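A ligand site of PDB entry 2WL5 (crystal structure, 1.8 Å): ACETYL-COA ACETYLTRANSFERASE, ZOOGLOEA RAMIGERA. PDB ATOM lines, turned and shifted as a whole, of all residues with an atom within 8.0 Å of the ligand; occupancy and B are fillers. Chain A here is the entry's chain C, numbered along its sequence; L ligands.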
ATOM      1  N   VAL A 276       9.805  16.066  16.122  1.00  0.00           N
ATOM      2  CA  VAL A 276       9.395  14.681  16.319  1.00  0.00           C
ATOM      3  C   VAL A 276       8.730  14.108  15.063  1.00  0.00           C
ATOM      4  O   VAL A 276       8.470  12.911  14.990  1.00  0.00           O
ATOM      5  CB  VAL A 276       8.453  14.491  17.544  1.00  0.00           C
ATOM      6  CG1 VAL A 276       8.986  15.245  18.751  1.00  0.00           C
ATOM      7  CG2 VAL A 276       7.036  14.947  17.215  1.00  0.00           C
ATOM      8  N   SER A 277       8.488  14.970  14.067  1.00  0.00           N
ATOM      9  CA  SER A 277       7.867  14.562  12.816  1.00  0.00           C
ATOM     10  C   SER A 277       7.453  15.740  11.926  1.00  0.00           C
ATOM     11  O   SER A 277       7.533  16.914  12.319  1.00  0.00           O
ATOM     12  CB  SER A 277       6.618  13.717  13.083  1.00  0.00           C
ATOM     13  OG  SER A 277       5.490  14.541  13.274  1.00  0.00           O
ATOM     14  N   LYS A 298      -1.428  13.939   9.433  1.00  0.00           N
ATOM     15  CA  LYS A 298      -0.386  12.935   9.231  1.00  0.00           C
ATOM     16  C   LYS A 298       0.749  13.188  10.210  1.00  0.00           C
ATOM     17  O   LYS A 298       1.253  12.265  10.842  1.00  0.00           O
ATOM     18  CB  LYS A 298       0.119  12.939   7.783  1.00  0.00           C
ATOM     19  CG  LYS A 298       0.597  11.574   7.299  1.00  0.00           C
ATOM     20  CD  LYS A 298       1.835  11.094   8.069  1.00  0.00           C
ATOM     21  CE  LYS A 298       2.105   9.606   7.827  1.00  0.00           C
ATOM     22  NZ  LYS A 298       2.575   9.317   6.439  1.00  0.00           N
ATOM     23  N   ALA A 299       1.143  14.453  10.348  1.00  0.00           N
ATOM     24  CA  ALA A 299       2.144  14.823  11.349  1.00  0.00           C
ATOM     25  C   ALA A 299       1.776  14.223  12.697  1.00  0.00           C
ATOM     26  O   ALA A 299       2.622  13.654  13.383  1.00  0.00           O
ATOM     27  CB  ALA A 299       2.266  16.328  11.449  1.00  0.00           C
ATOM     28  N   LEU A 300       0.504  14.355  13.064  1.00  0.00           N
ATOM     29  CA  LEU A 300       0.037  13.863  14.354  1.00  0.00           C
ATOM     30  C   LEU A 300       0.158  12.341  14.440  1.00  0.00           C
ATOM     31  O   LEU A 300       0.517  11.793  15.482  1.00  0.00           O
ATOM     32  CB  LEU A 300      -1.398  14.296  14.604  1.00  0.00           C
ATOM     33  CG  LEU A 300      -1.595  15.813  14.772  1.00  0.00           C
ATOM     34  CD1 LEU A 300      -3.052  16.194  14.601  1.00  0.00           C
ATOM     35  CD2 LEU A 300      -1.066  16.274  16.116  1.00  0.00           C
ATOM     36  N   GLU A 301      -0.123  11.668  13.323  1.00  0.00           N
ATOM     37  CA  GLU A 301      -0.096  10.218  13.280  1.00  0.00           C
ATOM     38  C   GLU A 301       1.337   9.698  13.350  1.00  0.00           C
ATOM     39  O   GLU A 301       1.598   8.633  13.927  1.00  0.00           O
ATOM     40  CB  GLU A 301      -0.773   9.701  12.001  1.00  0.00           C
ATOM     41  CG  GLU A 301      -0.801   8.185  11.884  1.00  0.00           C
ATOM     42  CD  GLU A 301      -1.651   7.698  10.714  1.00  0.00           C
ATOM     43  OE1 GLU A 301      -1.888   8.486   9.771  1.00  0.00           O
ATOM     44  OE2 GLU A 301      -2.061   6.515  10.735  1.00  0.00           O
ATOM     45  N   ARG A 302       2.257  10.464  12.775  1.00  0.00           N
ATOM     46  CA  ARG A 302       3.672  10.107  12.818  1.00  0.00           C
ATOM     47  C   ARG A 302       4.231  10.282  14.225  1.00  0.00           C
ATOM     48  O   ARG A 302       4.780   9.347  14.805  1.00  0.00           O
ATOM     49  CB  ARG A 302       4.469  10.923  11.792  1.00  0.00           C
ATOM     50  CG  ARG A 302       4.498  10.275  10.416  1.00  0.00           C
ATOM     51  CD  ARG A 302       5.222  11.124   9.376  1.00  0.00           C
ATOM     52  NE  ARG A 302       5.272  10.450   8.078  1.00  0.00           N
ATOM     53  CZ  ARG A 302       5.471  11.076   6.919  1.00  0.00           C
ATOM     54  NH1 ARG A 302       5.610  12.394   6.890  1.00  0.00           N
ATOM     55  NH2 ARG A 302       5.501  10.387   5.787  1.00  0.00           N
ATOM     56  N   ALA A 303       4.064  11.485  14.770  1.00  0.00           N
ATOM     57  CA  ALA A 303       4.473  11.750  16.148  1.00  0.00           C
ATOM     58  C   ALA A 303       3.619  10.920  17.105  1.00  0.00           C
ATOM     59  O   ALA A 303       3.952  10.765  18.270  1.00  0.00           O
ATOM     60  CB  ALA A 303       4.340  13.215  16.466  1.00  0.00           C
ATOM     61  N   GLY A 304       2.510  10.396  16.585  1.00  0.00           N
ATOM     62  CA  GLY A 304       1.594   9.603  17.386  1.00  0.00           C
ATOM     63  C   GLY A 304       0.803  10.459  18.350  1.00  0.00           C
ATOM     64  O   GLY A 304       0.143   9.933  19.257  1.00  0.00           O
ATOM     65  N   TRP A 305       0.852  11.772  18.169  1.00  0.00           N
ATOM     66  CA  TRP A 305       0.103  12.690  19.028  1.00  0.00           C
ATOM     67  C   TRP A 305      -1.385  12.711  18.678  1.00  0.00           C
ATOM     68  O   TRP A 305      -1.775  12.363  17.565  1.00  0.00           O
ATOM     69  CB  TRP A 305       0.672  14.105  18.939  1.00  0.00           C
ATOM     70  CG  TRP A 305       2.013  14.266  19.585  1.00  0.00           C
ATOM     71  CD1 TRP A 305       2.615  13.403  20.443  1.00  0.00           C
ATOM     72  CD2 TRP A 305       2.898  15.377  19.442  1.00  0.00           C
ATOM     73  NE1 TRP A 305       3.841  13.900  20.828  1.00  0.00           N
ATOM     74  CE2 TRP A 305       4.037  15.107  20.228  1.00  0.00           C
ATOM     75  CE3 TRP A 305       2.854  16.581  18.716  1.00  0.00           C
ATOM     76  CZ2 TRP A 305       5.113  15.995  20.319  1.00  0.00           C
ATOM     77  CZ3 TRP A 305       3.919  17.451  18.803  1.00  0.00           C
ATOM     78  CH2 TRP A 305       5.036  17.151  19.609  1.00  0.00           C
ATOM     79  N   LYS A 306      -2.191  13.129  19.647  1.00  0.00           N
ATOM     80  CA  LYS A 306      -3.626  13.290  19.457  1.00  0.00           C
ATOM     81  C   LYS A 306      -3.961  14.778  19.404  1.00  0.00           C
ATOM     82  O   LYS A 306      -3.299  15.582  20.048  1.00  0.00           O
ATOM     83  CB  LYS A 306      -4.374  12.604  20.598  1.00  0.00           C
ATOM     84  CG  LYS A 306      -4.009  11.133  20.734  1.00  0.00           C
ATOM     85  CD  LYS A 306      -3.723  10.746  22.174  1.00  0.00           C
ATOM     86  CE  LYS A 306      -3.078   9.374  22.257  1.00  0.00           C
ATOM     87  NZ  LYS A 306      -2.494   9.107  23.595  1.00  0.00           N
HETATM   88  C1  LIG L   1       1.866   5.279  15.069  1.00  0.00           C
HETATM   89  C2  LIG L   1       2.732   5.514  16.303  1.00  0.00           C
HETATM   90  C3  LIG L   1       3.708   6.736  16.177  1.00  0.00           C
HETATM   91  C4  LIG L   1       4.631   6.993  17.491  1.00  0.00           C
HETATM   92  C5  LIG L   1       6.124   6.782  17.267  1.00  0.00           C
HETATM   93  C6  LIG L   1       6.954   7.303  18.387  1.00  0.00           C
HETATM   94  O1  LIG L   1       0.931   6.238  14.740  1.00  0.00           O
HETATM   95  O2  LIG L   1       1.993   5.493  17.530  1.00  0.00           O
HETATM   96  O3  LIG L   1       4.444   6.707  14.969  1.00  0.00           O
HETATM   97  O4  LIG L   1       4.327   8.145  18.246  1.00  0.00           O
HETATM   98  O5  LIG L   1       6.483   5.470  16.832  1.00  0.00           O
HETATM   99  O6  LIG L   1       6.721   6.780  19.706  1.00  0.00           O
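An oxygen (O1) of the ligand sits close to the backbone carbonyl oxygen of Glu 301. An oxygen (O4) of the ligand lies within hydrogen-bond range of the backbone carbonyl oxygen (O) of Ala 303 (2.6 Å). An oxygen (O3) of the ligand is in hydrogen-bond range of the backbone carbonyl oxygen (O) of Arg 302 (2.7 Å). The backbone NH (N) of Gly 304 sits close to an oxygen (O4) of the ligand (3.3 Å).
Four residues have an atom within 4 Å of the ligand: Glu 301, Arg 302, Ala 303 and Gly 304. The nearest printed residue that does not touch the ligand is Trp 305 (5.0 Å).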
